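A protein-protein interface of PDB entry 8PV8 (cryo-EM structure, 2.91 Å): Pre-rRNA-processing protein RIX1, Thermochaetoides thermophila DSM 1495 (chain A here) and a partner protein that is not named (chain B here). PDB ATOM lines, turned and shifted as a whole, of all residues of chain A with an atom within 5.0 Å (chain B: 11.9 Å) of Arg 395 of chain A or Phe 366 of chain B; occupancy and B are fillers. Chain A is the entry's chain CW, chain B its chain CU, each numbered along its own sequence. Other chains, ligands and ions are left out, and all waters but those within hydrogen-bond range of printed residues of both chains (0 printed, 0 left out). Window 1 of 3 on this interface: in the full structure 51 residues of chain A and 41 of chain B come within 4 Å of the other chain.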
ATOM      1  N   TYR A 323      -3.724   9.791  -2.640  1.00  0.00           N
ATOM      2  CA  TYR A 323      -3.855   9.271  -4.002  1.00  0.00           C
ATOM      3  C   TYR A 323      -2.503   9.127  -4.686  1.00  0.00           C
ATOM      4  O   TYR A 323      -2.269   8.143  -5.396  1.00  0.00           O
ATOM      5  CB  TYR A 323      -4.754  10.160  -4.863  1.00  0.00           C
ATOM      6  CG  TYR A 323      -6.225   9.854  -4.757  1.00  0.00           C
ATOM      7  CD1 TYR A 323      -7.059  10.640  -3.986  1.00  0.00           C
ATOM      8  CD2 TYR A 323      -6.775   8.759  -5.408  1.00  0.00           C
ATOM      9  CE1 TYR A 323      -8.394  10.368  -3.879  1.00  0.00           C
ATOM     10  CE2 TYR A 323      -8.119   8.473  -5.304  1.00  0.00           C
ATOM     11  CZ  TYR A 323      -8.922   9.283  -4.533  1.00  0.00           C
ATOM     12  OH  TYR A 323     -10.263   9.020  -4.411  1.00  0.00           O
ATOM     13  N   PHE A 324      -1.606  10.088  -4.492  1.00  0.00           N
ATOM     14  CA  PHE A 324      -0.258   9.993  -5.029  1.00  0.00           C
ATOM     15  C   PHE A 324       0.666   9.167  -4.150  1.00  0.00           C
ATOM     16  O   PHE A 324       1.745   8.778  -4.605  1.00  0.00           O
ATOM     17  CB  PHE A 324       0.330  11.391  -5.227  1.00  0.00           C
ATOM     18  CG  PHE A 324      -0.275  12.137  -6.373  1.00  0.00           C
ATOM     19  CD1 PHE A 324      -1.396  12.926  -6.186  1.00  0.00           C
ATOM     20  CD2 PHE A 324       0.265  12.034  -7.642  1.00  0.00           C
ATOM     21  CE1 PHE A 324      -1.960  13.607  -7.241  1.00  0.00           C
ATOM     22  CE2 PHE A 324      -0.294  12.715  -8.702  1.00  0.00           C
ATOM     23  CZ  PHE A 324      -1.408  13.502  -8.500  1.00  0.00           C
ATOM     24  N   ASN A 325       0.280   8.905  -2.904  1.00  0.00           N
ATOM     25  CA  ASN A 325       1.052   8.018  -2.046  1.00  0.00           C
ATOM     26  C   ASN A 325       0.655   6.551  -2.154  1.00  0.00           C
ATOM     27  O   ASN A 325       1.340   5.703  -1.573  1.00  0.00           O
ATOM     28  CB  ASN A 325       0.941   8.463  -0.581  1.00  0.00           C
ATOM     29  CG  ASN A 325       1.820   9.655  -0.271  1.00  0.00           C
ATOM     30  OD1 ASN A 325       2.680  10.027  -1.069  1.00  0.00           O
ATOM     31  ND2 ASN A 325       1.610  10.260   0.890  1.00  0.00           N
ATOM     32  N   ASN A 326      -0.425   6.220  -2.878  1.00  0.00           N
ATOM     33  CA  ASN A 326      -0.804   4.815  -2.988  1.00  0.00           C
ATOM     34  C   ASN A 326      -0.672   4.310  -4.424  1.00  0.00           C
ATOM     35  O   ASN A 326      -0.915   5.058  -5.377  1.00  0.00           O
ATOM     36  CB  ASN A 326      -2.241   4.587  -2.505  1.00  0.00           C
ATOM     37  CG  ASN A 326      -2.417   4.911  -1.042  1.00  0.00           C
ATOM     38  OD1 ASN A 326      -1.906   4.202  -0.177  1.00  0.00           O
ATOM     39  ND2 ASN A 326      -3.146   5.979  -0.753  1.00  0.00           N
ATOM     40  N   PRO A 327      -0.297   3.044  -4.610  1.00  0.00           N
ATOM     41  CA  PRO A 327      -0.128   2.509  -5.967  1.00  0.00           C
ATOM     42  C   PRO A 327      -1.459   2.148  -6.608  1.00  0.00           C
ATOM     43  O   PRO A 327      -2.515   2.122  -5.973  1.00  0.00           O
ATOM     44  CB  PRO A 327       0.735   1.265  -5.744  1.00  0.00           C
ATOM     45  CG  PRO A 327       0.380   0.827  -4.374  1.00  0.00           C
ATOM     46  CD  PRO A 327       0.179   2.094  -3.590  1.00  0.00           C
ATOM     47  N   ALA A 391       4.040  15.618  -2.736  1.00  0.00           N
ATOM     48  CA  ALA A 391       3.720  14.243  -3.118  1.00  0.00           C
ATOM     49  C   ALA A 391       3.644  14.083  -4.633  1.00  0.00           C
ATOM     50  O   ALA A 391       4.090  13.064  -5.178  1.00  0.00           O
ATOM     51  CB  ALA A 391       2.409  13.808  -2.472  1.00  0.00           C
ATOM     52  N   ILE A 392       3.072  15.075  -5.325  1.00  0.00           N
ATOM     53  CA  ILE A 392       3.023  15.047  -6.786  1.00  0.00           C
ATOM     54  C   ILE A 392       4.431  15.052  -7.370  1.00  0.00           C
ATOM     55  O   ILE A 392       4.735  14.290  -8.297  1.00  0.00           O
ATOM     56  CB  ILE A 392       2.185  16.225  -7.317  1.00  0.00           C
ATOM     57  CG1 ILE A 392       0.706  16.024  -6.992  1.00  0.00           C
ATOM     58  CG2 ILE A 392       2.368  16.402  -8.817  1.00  0.00           C
ATOM     59  CD1 ILE A 392      -0.181  17.149  -7.478  1.00  0.00           C
ATOM     60  N   ILE A 393       5.310  15.899  -6.826  1.00  0.00           N
ATOM     61  CA  ILE A 393       6.697  15.959  -7.278  1.00  0.00           C
ATOM     62  C   ILE A 393       7.393  14.621  -7.057  1.00  0.00           C
ATOM     63  O   ILE A 393       8.086  14.114  -7.948  1.00  0.00           O
ATOM     64  CB  ILE A 393       7.435  17.106  -6.560  1.00  0.00           C
ATOM     65  CG1 ILE A 393       6.944  18.472  -7.053  1.00  0.00           C
ATOM     66  CG2 ILE A 393       8.936  16.967  -6.720  1.00  0.00           C
ATOM     67  CD1 ILE A 393       7.513  18.917  -8.368  1.00  0.00           C
ATOM     68  N   ARG A 394       7.190  14.012  -5.883  1.00  0.00           N
ATOM     69  CA  ARG A 394       7.837  12.740  -5.574  1.00  0.00           C
ATOM     70  C   ARG A 394       7.361  11.620  -6.490  1.00  0.00           C
ATOM     71  O   ARG A 394       8.167  10.795  -6.934  1.00  0.00           O
ATOM     72  CB  ARG A 394       7.591  12.367  -4.114  1.00  0.00           C
ATOM     73  CG  ARG A 394       8.451  11.215  -3.624  1.00  0.00           C
ATOM     74  CD  ARG A 394       8.292  11.002  -2.130  1.00  0.00           C
ATOM     75  NE  ARG A 394       6.963  11.379  -1.665  1.00  0.00           N
ATOM     76  CZ  ARG A 394       6.532  11.214  -0.422  1.00  0.00           C
ATOM     77  NH1 ARG A 394       7.301  10.675   0.510  1.00  0.00           N
ATOM     78  NH2 ARG A 394       5.299  11.600  -0.106  1.00  0.00           N
ATOM     79  N   ARG A 395       6.062  11.568  -6.786  1.00  0.00           N
ATOM     80  CA  ARG A 395       5.550  10.471  -7.603  1.00  0.00           C
ATOM     81  C   ARG A 395       5.880  10.661  -9.084  1.00  0.00           C
ATOM     82  O   ARG A 395       6.212   9.697  -9.781  1.00  0.00           O
ATOM     83  CB  ARG A 395       4.041  10.312  -7.380  1.00  0.00           C
ATOM     84  CG  ARG A 395       3.358   9.225  -8.212  1.00  0.00           C
ATOM     85  CD  ARG A 395       4.070   7.869  -8.174  1.00  0.00           C
ATOM     86  NE  ARG A 395       4.248   7.311  -6.840  1.00  0.00           N
ATOM     87  CZ  ARG A 395       3.322   6.629  -6.180  1.00  0.00           C
ATOM     88  NH1 ARG A 395       2.107   6.466  -6.668  1.00  0.00           N
ATOM     89  NH2 ARG A 395       3.623   6.101  -4.998  1.00  0.00           N
ATOM     90  N   LEU A 396       5.819  11.897  -9.588  1.00  0.00           N
ATOM     91  CA  LEU A 396       6.005  12.084 -11.024  1.00  0.00           C
ATOM     92  C   LEU A 396       7.473  12.231 -11.408  1.00  0.00           C
ATOM     93  O   LEU A 396       7.854  11.827 -12.514  1.00  0.00           O
ATOM     94  CB  LEU A 396       5.208  13.292 -11.514  1.00  0.00           C
ATOM     95  CG  LEU A 396       3.701  13.293 -11.252  1.00  0.00           C
ATOM     96  CD1 LEU A 396       3.042  14.438 -11.998  1.00  0.00           C
ATOM     97  CD2 LEU A 396       3.073  11.966 -11.639  1.00  0.00           C
ATOM     98  N   GLU A 397       8.298  12.803 -10.521  1.00  0.00           N
ATOM     99  CA  GLU A 397       9.727  13.064 -10.743  1.00  0.00           C
ATOM    100  C   GLU A 397       9.873  13.967 -11.963  1.00  0.00           C
ATOM    101  O   GLU A 397       9.364  15.100 -11.929  1.00  0.00           O
ATOM    102  CB  GLU A 397      10.498  11.742 -10.794  1.00  0.00           C
ATOM    103  CG  GLU A 397      10.573  11.022  -9.462  1.00  0.00           C
ATOM    104  CD  GLU A 397      11.440   9.782  -9.521  1.00  0.00           C
ATOM    105  OE1 GLU A 397      11.928   9.449 -10.621  1.00  0.00           O
ATOM    106  OE2 GLU A 397      11.633   9.139  -8.467  1.00  0.00           O
ATOM    107  N   GLY B  96      13.906  10.091 -20.413  1.00  0.00           N
ATOM    108  CA  GLY B  96      12.837   9.853 -19.463  1.00  0.00           C
ATOM    109  C   GLY B  96      11.552   9.426 -20.153  1.00  0.00           C
ATOM    110  O   GLY B  96      11.457   8.345 -20.736  1.00  0.00           O
ATOM    111  N   ASP B  97      10.547  10.296 -20.079  1.00  0.00           N
ATOM    112  CA  ASP B  97       9.241  10.035 -20.684  1.00  0.00           C
ATOM    113  C   ASP B  97       8.923  10.990 -21.825  1.00  0.00           C
ATOM    114  O   ASP B  97       7.755  11.160 -22.200  1.00  0.00           O
ATOM    115  CB  ASP B  97       8.160  10.093 -19.613  1.00  0.00           C
ATOM    116  CG  ASP B  97       8.252   8.942 -18.633  1.00  0.00           C
ATOM    117  OD1 ASP B  97       8.725   7.858 -19.037  1.00  0.00           O
ATOM    118  OD2 ASP B  97       7.848   9.115 -17.466  1.00  0.00           O
ATOM    119  N   CYS B 114       3.707   9.867 -22.186  1.00  0.00           N
ATOM    120  CA  CYS B 114       2.706   9.520 -21.184  1.00  0.00           C
ATOM    121  C   CYS B 114       1.456  10.384 -21.314  1.00  0.00           C
ATOM    122  O   CYS B 114       0.336   9.896 -21.127  1.00  0.00           O
ATOM    123  CB  CYS B 114       3.299   9.643 -19.784  1.00  0.00           C
ATOM    124  SG  CYS B 114       4.786   8.657 -19.515  1.00  0.00           S
ATOM    125  N   THR B 115       1.620  11.669 -21.624  1.00  0.00           N
ATOM    126  CA  THR B 115       0.475  12.566 -21.708  1.00  0.00           C
ATOM    127  C   THR B 115      -0.025  12.763 -23.132  1.00  0.00           C
ATOM    128  O   THR B 115      -1.140  13.263 -23.315  1.00  0.00           O
ATOM    129  CB  THR B 115       0.814  13.935 -21.111  1.00  0.00           C
ATOM    130  OG1 THR B 115       1.847  14.549 -21.882  1.00  0.00           O
ATOM    131  CG2 THR B 115       1.309  13.780 -19.684  1.00  0.00           C
ATOM    132  N   SER B 337      14.748   1.552 -10.132  1.00  0.00           N
ATOM    133  CA  SER B 337      13.461   1.749  -9.481  1.00  0.00           C
ATOM    134  C   SER B 337      12.858   3.074  -9.925  1.00  0.00           C
ATOM    135  O   SER B 337      13.452   4.137  -9.714  1.00  0.00           O
ATOM    136  CB  SER B 337      13.615   1.717  -7.961  1.00  0.00           C
ATOM    137  OG  SER B 337      14.455   2.764  -7.512  1.00  0.00           O
ATOM    138  N   LYS B 338      11.681   3.005 -10.539  1.00  0.00           N
ATOM    139  CA  LYS B 338      10.968   4.175 -11.016  1.00  0.00           C
ATOM    140  C   LYS B 338       9.550   4.152 -10.460  1.00  0.00           C
ATOM    141  O   LYS B 338       8.877   3.116 -10.525  1.00  0.00           O
ATOM    142  CB  LYS B 338      10.938   4.208 -12.551  1.00  0.00           C
ATOM    143  CG  LYS B 338      10.307   5.454 -13.147  1.00  0.00           C
ATOM    144  CD  LYS B 338      10.393   5.445 -14.664  1.00  0.00           C
ATOM    145  CE  LYS B 338       9.753   6.689 -15.257  1.00  0.00           C
ATOM    146  NZ  LYS B 338       9.823   6.701 -16.744  1.00  0.00           N
ATOM    147  N   PRO B 339       9.078   5.266  -9.888  1.00  0.00           N
ATOM    148  CA  PRO B 339       7.746   5.272  -9.261  1.00  0.00           C
ATOM    149  C   PRO B 339       6.588   5.087 -10.231  1.00  0.00           C
ATOM    150  O   PRO B 339       5.486   4.749  -9.782  1.00  0.00           O
ATOM    151  CB  PRO B 339       7.682   6.648  -8.586  1.00  0.00           C
ATOM    152  CG  PRO B 339       8.676   7.479  -9.321  1.00  0.00           C
ATOM    153  CD  PRO B 339       9.779   6.548  -9.705  1.00  0.00           C
ATOM    154  N   THR B 340       6.788   5.299 -11.530  1.00  0.00           N
ATOM    155  CA  THR B 340       5.731   5.114 -12.512  1.00  0.00           C
ATOM    156  C   THR B 340       6.216   4.179 -13.610  1.00  0.00           C
ATOM    157  O   THR B 340       7.384   4.203 -14.004  1.00  0.00           O
ATOM    158  CB  THR B 340       5.280   6.445 -13.131  1.00  0.00           C
ATOM    159  OG1 THR B 340       6.405   7.107 -13.720  1.00  0.00           O
ATOM    160  CG2 THR B 340       4.654   7.347 -12.080  1.00  0.00           C
ATOM    161  N   LYS B 341       5.301   3.350 -14.102  1.00  0.00           N
ATOM    162  CA  LYS B 341       5.561   2.465 -15.229  1.00  0.00           C
ATOM    163  C   LYS B 341       4.645   2.846 -16.382  1.00  0.00           C
ATOM    164  O   LYS B 341       3.436   3.006 -16.192  1.00  0.00           O
ATOM    165  CB  LYS B 341       5.354   0.995 -14.852  1.00  0.00           C
ATOM    166  CG  LYS B 341       5.738   0.028 -15.963  1.00  0.00           C
ATOM    167  CD  LYS B 341       5.463  -1.420 -15.590  1.00  0.00           C
ATOM    168  CE  LYS B 341       6.472  -1.933 -14.580  1.00  0.00           C
ATOM    169  NZ  LYS B 341       6.283  -3.383 -14.297  1.00  0.00           N
ATOM    170  N   THR B 342       5.226   2.992 -17.574  1.00  0.00           N
ATOM    171  CA  THR B 342       4.464   3.333 -18.773  1.00  0.00           C
ATOM    172  C   THR B 342       4.115   2.038 -19.502  1.00  0.00           C
ATOM    173  O   THR B 342       4.807   1.592 -20.420  1.00  0.00           O
ATOM    174  CB  THR B 342       5.255   4.286 -19.659  1.00  0.00           C
ATOM    175  OG1 THR B 342       5.793   5.345 -18.860  1.00  0.00           O
ATOM    176  CG2 THR B 342       4.358   4.882 -20.733  1.00  0.00           C
ATOM    177  N   PHE B 357      -2.124  12.819 -17.090  1.00  0.00           N
ATOM    178  CA  PHE B 357      -0.929  11.989 -17.019  1.00  0.00           C
ATOM    179  C   PHE B 357      -1.344  10.533 -16.881  1.00  0.00           C
ATOM    180  O   PHE B 357      -2.119  10.188 -15.982  1.00  0.00           O
ATOM    181  CB  PHE B 357      -0.048  12.406 -15.841  1.00  0.00           C
ATOM    182  CG  PHE B 357       1.248  11.657 -15.753  1.00  0.00           C
ATOM    183  CD1 PHE B 357       2.264  11.896 -16.660  1.00  0.00           C
ATOM    184  CD2 PHE B 357       1.450  10.719 -14.756  1.00  0.00           C
ATOM    185  CE1 PHE B 357       3.458  11.209 -16.577  1.00  0.00           C
ATOM    186  CE2 PHE B 357       2.641  10.031 -14.668  1.00  0.00           C
ATOM    187  CZ  PHE B 357       3.645  10.275 -15.580  1.00  0.00           C
ATOM    188  N   THR B 358      -0.827   9.682 -17.764  1.00  0.00           N
ATOM    189  CA  THR B 358      -1.216   8.279 -17.830  1.00  0.00           C
ATOM    190  C   THR B 358      -0.016   7.399 -17.509  1.00  0.00           C
ATOM    191  O   THR B 358       0.879   7.238 -18.346  1.00  0.00           O
ATOM    192  CB  THR B 358      -1.762   7.927 -19.214  1.00  0.00           C
ATOM    193  OG1 THR B 358      -0.702   8.008 -20.173  1.00  0.00           O
ATOM    194  CG2 THR B 358      -2.868   8.891 -19.612  1.00  0.00           C
ATOM    195  N   ALA B 359      -0.007   6.824 -16.307  1.00  0.00           N
ATOM    196  CA  ALA B 359       1.014   5.862 -15.920  1.00  0.00           C
ATOM    197  C   ALA B 359       0.477   5.005 -14.786  1.00  0.00           C
ATOM    198  O   ALA B 359      -0.457   5.391 -14.080  1.00  0.00           O
ATOM    199  CB  ALA B 359       2.317   6.550 -15.499  1.00  0.00           C
ATOM    200  N   GLN B 360       1.085   3.833 -14.620  1.00  0.00           N
ATOM    201  CA  GLN B 360       0.756   2.922 -13.533  1.00  0.00           C
ATOM    202  C   GLN B 360       1.640   3.241 -12.338  1.00  0.00           C
ATOM    203  O   GLN B 360       2.868   3.298 -12.466  1.00  0.00           O
ATOM    204  CB  GLN B 360       0.936   1.462 -13.957  1.00  0.00           C
ATOM    205  CG  GLN B 360       0.935   0.476 -12.801  1.00  0.00           C
ATOM    206  CD  GLN B 360       0.723  -0.954 -13.250  1.00  0.00           C
ATOM    207  OE1 GLN B 360       0.534  -1.223 -14.435  1.00  0.00           O
ATOM    208  NE2 GLN B 360       0.754  -1.883 -12.304  1.00  0.00           N
ATOM    209  N   PHE B 361       1.016   3.447 -11.184  1.00  0.00           N
ATOM    210  CA  PHE B 361       1.737   3.843  -9.982  1.00  0.00           C
ATOM    211  C   PHE B 361       2.390   2.623  -9.346  1.00  0.00           C
ATOM    212  O   PHE B 361       1.699   1.702  -8.896  1.00  0.00           O
ATOM    213  CB  PHE B 361       0.783   4.524  -9.004  1.00  0.00           C
ATOM    214  CG  PHE B 361       0.476   5.955  -9.351  1.00  0.00           C
ATOM    215  CD1 PHE B 361       1.139   6.593 -10.387  1.00  0.00           C
ATOM    216  CD2 PHE B 361      -0.479   6.661  -8.641  1.00  0.00           C
ATOM    217  CE1 PHE B 361       0.856   7.903 -10.704  1.00  0.00           C
ATOM    218  CE2 PHE B 361      -0.764   7.973  -8.954  1.00  0.00           C
ATOM    219  CZ  PHE B 361      -0.097   8.594  -9.987  1.00  0.00           C
ATOM    220  N   GLU B 362       3.720   2.614  -9.312  1.00  0.00           N
ATOM    221  CA  GLU B 362       4.466   1.502  -8.755  1.00  0.00           C
ATOM    222  C   GLU B 362       4.470   1.572  -7.230  1.00  0.00           C
ATOM    223  O   GLU B 362       4.401   2.656  -6.646  1.00  0.00           O
ATOM    224  CB  GLU B 362       5.892   1.502  -9.303  1.00  0.00           C
ATOM    225  CG  GLU B 362       5.970   1.085 -10.756  1.00  0.00           C
ATOM    226  CD  GLU B 362       5.672  -0.385 -10.944  1.00  0.00           C
ATOM    227  OE1 GLU B 362       6.073  -1.190 -10.079  1.00  0.00           O
ATOM    228  OE2 GLU B 362       5.015  -0.733 -11.946  1.00  0.00           O
ATOM    229  N   PRO B 363       4.543   0.420  -6.551  1.00  0.00           N
ATOM    230  CA  PRO B 363       4.622   0.439  -5.084  1.00  0.00           C
ATOM    231  C   PRO B 363       6.008   0.801  -4.576  1.00  0.00           C
ATOM    232  O   PRO B 363       6.914  -0.037  -4.572  1.00  0.00           O
ATOM    233  CB  PRO B 363       4.239  -0.995  -4.685  1.00  0.00           C
ATOM    234  CG  PRO B 363       3.799  -1.678  -5.945  1.00  0.00           C
ATOM    235  CD  PRO B 363       4.430  -0.949  -7.075  1.00  0.00           C
ATOM    236  N   MET B 364       6.170   2.041  -4.117  1.00  0.00           N
ATOM    237  CA  MET B 364       7.459   2.548  -3.664  1.00  0.00           C
ATOM    238  C   MET B 364       7.560   2.654  -2.149  1.00  0.00           C
ATOM    239  O   MET B 364       8.580   3.141  -1.647  1.00  0.00           O
ATOM    240  CB  MET B 364       7.741   3.915  -4.292  1.00  0.00           C
ATOM    241  CG  MET B 364       8.100   3.944  -5.789  1.00  0.00           C
ATOM    242  SD  MET B 364       9.564   3.042  -6.384  1.00  0.00           S
ATOM    243  CE  MET B 364       8.962   1.385  -6.713  1.00  0.00           C
ATOM    244  N   SER B 365       6.531   2.203  -1.419  1.00  0.00           N
ATOM    245  CA  SER B 365       6.498   2.220   0.049  1.00  0.00           C
ATOM    246  C   SER B 365       6.703   3.629   0.605  1.00  0.00           C
ATOM    247  O   SER B 365       7.511   3.849   1.509  1.00  0.00           O
ATOM    248  CB  SER B 365       7.521   1.246   0.641  1.00  0.00           C
ATOM    249  OG  SER B 365       8.816   1.822   0.646  1.00  0.00           O
ATOM    250  N   PHE B 366       5.979   4.598   0.039  1.00  0.00           N
ATOM    251  CA  PHE B 366       6.076   5.971   0.523  1.00  0.00           C
ATOM    252  C   PHE B 366       5.389   6.131   1.873  1.00  0.00           C
ATOM    253  O   PHE B 366       5.771   6.993   2.673  1.00  0.00           O
ATOM    254  CB  PHE B 366       5.479   6.937  -0.500  1.00  0.00           C
ATOM    255  CG  PHE B 366       6.336   7.141  -1.715  1.00  0.00           C
ATOM    256  CD1 PHE B 366       5.764   7.367  -2.955  1.00  0.00           C
ATOM    257  CD2 PHE B 366       7.717   7.105  -1.617  1.00  0.00           C
ATOM    258  CE1 PHE B 366       6.551   7.554  -4.077  1.00  0.00           C
ATOM    259  CE2 PHE B 366       8.510   7.291  -2.735  1.00  0.00           C
ATOM    260  CZ  PHE B 366       7.926   7.516  -3.966  1.00  0.00           C
ATOM    261  N   THR B 367       4.377   5.313   2.146  1.00  0.00           N
ATOM    262  CA  THR B 367       3.630   5.368   3.394  1.00  0.00           C
ATOM    263  C   THR B 367       4.192   4.339   4.364  1.00  0.00           C
ATOM    264  O   THR B 367       4.334   3.162   4.015  1.00  0.00           O
ATOM    265  CB  THR B 367       2.140   5.110   3.156  1.00  0.00           C
ATOM    266  N   LYS B 368       4.510   4.783   5.578  1.00  0.00           N
ATOM    267  CA  LYS B 368       5.057   3.922   6.617  1.00  0.00           C
ATOM    268  C   LYS B 368       4.263   4.101   7.902  1.00  0.00           C
ATOM    269  O   LYS B 368       3.865   5.219   8.248  1.00  0.00           O
ATOM    270  CB  LYS B 368       6.537   4.229   6.867  1.00  0.00           C
ATOM    271  N   SER B 369       4.038   2.996   8.608  1.00  0.00           N
ATOM    272  CA  SER B 369       3.297   3.000   9.859  1.00  0.00           C
ATOM    273  C   SER B 369       4.081   2.235  10.915  1.00  0.00           C
ATOM    274  O   SER B 369       5.084   1.579  10.619  1.00  0.00           O
ATOM    275  CB  SER B 369       1.902   2.384   9.690  1.00  0.00           C
ATOM    276  N   ARG B 370       3.616   2.336  12.163  1.00  0.00           N
ATOM    277  CA  ARG B 370       4.273   1.617  13.249  1.00  0.00           C
ATOM    278  C   ARG B 370       4.032   0.116  13.143  1.00  0.00           C
ATOM    279  O   ARG B 370       4.885  -0.684  13.543  1.00  0.00           O
ATOM    280  CB  ARG B 370       3.802   2.153  14.604  1.00  0.00           C
ATOM    281  CG  ARG B 370       2.324   1.953  14.898  1.00  0.00           C
ATOM    282  CD  ARG B 370       1.996   2.276  16.341  1.00  0.00           C
ATOM    283  NE  ARG B 370       2.169   1.113  17.201  1.00  0.00           N
ATOM    284  CZ  ARG B 370       1.184   0.308  17.577  1.00  0.00           C
ATOM    285  NH1 ARG B 370      -0.063   0.511  17.183  1.00  0.00           N
ATOM    286  NH2 ARG B 370       1.457  -0.725  18.369  1.00  0.00           N
ATOM    287  N   ASP B 372       3.943  -1.526  10.404  1.00  0.00           N
ATOM    288  CA  ASP B 372       4.811  -2.054   9.359  1.00  0.00           C
ATOM    289  C   ASP B 372       6.081  -2.652   9.949  1.00  0.00           C
ATOM    290  O   ASP B 372       6.610  -3.637   9.422  1.00  0.00           O
ATOM    291  CB  ASP B 372       5.154  -0.956   8.355  1.00  0.00           C
ATOM    292  CG  ASP B 372       3.957  -0.520   7.537  1.00  0.00           C
ATOM    293  OD1 ASP B 372       3.062  -1.358   7.301  1.00  0.00           O
ATOM    294  OD2 ASP B 372       3.911   0.659   7.127  1.00  0.00           O
ATOM    295  N   ASN B 376       7.195  -6.465   9.126  1.00  0.00           N
ATOM    296  CA  ASN B 376       8.395  -6.872   8.402  1.00  0.00           C
ATOM    297  C   ASN B 376       9.559  -7.250   9.311  1.00  0.00           C
ATOM    298  O   ASN B 376      10.604  -7.673   8.807  1.00  0.00           O
ATOM    299  CB  ASN B 376       8.827  -5.781   7.401  1.00  0.00           C
ATOM    300  CG  ASN B 376       9.238  -4.460   8.061  1.00  0.00           C
ATOM    301  OD1 ASN B 376       9.328  -4.333   9.283  1.00  0.00           O
ATOM    302  ND2 ASN B 376       9.492  -3.460   7.227  1.00  0.00           N
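Among the printed residues, pairs that only touch across the chains: Tyr 323 of chain A with Phe 361 of chain B (3.9 Å), Asn 326 of chain A with Phe 361 of chain B (3.7 Å), Pro 327 of chain A with Phe 361 of chain B (3.3 Å), Pro 327 of chain A with Pro 363 of chain B (3.98 Å), Arg 394 of chain A with Phe 366 of chain B (3.8 Å), Arg 395 of chain A with Pro 339 of chain B (3.3 Å), Arg 395 of chain A with Thr 340 of chain B (3.6 Å), Arg 395 of chain A with Phe 361 of chain B (3.2 Å), Arg 395 of chain A with Glu 362 of chain B (3.9 Å), Arg 395 of chain A with Phe 366 of chain B (3.2 Å), Leu 396 of chain A with Phe 357 of chain B (3.6 Å) and Glu 397 of chain A with Pro 339 of chain B (3.4 Å).
Printed residues of chain B that touch a printed residue of chain A: Pro 339, Thr 340, Phe 357, Phe 361, Glu 362, Pro 363 and Phe 366.
Hydrophobic or aromatic side chains of chain B within 4 Å of the printed part of chain A: Pro 339, Phe 357, Phe 361 and Phe 366.
Printed residues of chain A that touch a printed residue of chain B: Tyr 323, Asn 326, Pro 327, Arg 394, Arg 395, Leu 396 and Glu 397.
Hydrophobic or aromatic side chains of chain A within 4 Å of the printed part of chain B: Pro 327 and Leu 396.
Of chain B, only Pro 339, Thr 340, Phe 361, Glu 362 and Phe 366 come within 4 Å of Arg 395 of chain A.
Phe 366 of chain B touches just these residues of chain A: Arg 394 (3.8 Å) and Arg 395 (3.2 Å).
No residue of chain B comes within 4 Å of Phe 324 of chain A.
No residue of chain B comes within 4 Å of Asn 325 of chain A.
No residue of chain B comes within 4 Å of Ala 391 of chain A.
Of chain B, only Phe 366 (3.8 Å) comes within 4 Å of Arg 394 of chain A.
Leu 396 of chain A touches one residue of chain B.
Glu 397 of chain A touches one residue of chain B.
Of the printed residues of chain B, Asn 326 of chain A touches Phe 361.
Of the printed residues of chain B, Tyr 323 of chain A touches Phe 361 (3.9 Å).
Printed residues of chain A within 4 Å of Thr 340 of chain B: Arg 395 (3.6 Å).
Printed residues of chain B within 4 Å of Pro 327 of chain A: Phe 361 (3.3 Å) and Pro 363 (3.98 Å).
Ala 359 of chain B touches none of the printed residues of chain A.
The nearest residue of chain A that does not touch Phe 366 of chain B is Asn 325 of chain A (4.2 Å).
The nearest printed residue of chain B that does not touch Pro 327 of chain A is Glu 362 of chain B (4.02 Å).
The backbone carbonyl oxygen (O) of Phe 324 of chain A lies close to the guanidinium group (NH1) of Arg 395 of chain A.
O of Pro 339 of chain B lies within hydrogen-bond range of N of Glu 362 of chain B (2.8 Å).
The side-chain amino group (NZ) of Lys 341 of chain B is in salt-bridge range of the side-chain carboxylate (OE2) of Glu 362 of chain B, 3.8 Å away.
OD1 of Asn 325 of chain A is in hydrogen-bond range of NH2 of Arg 394 of chain A.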
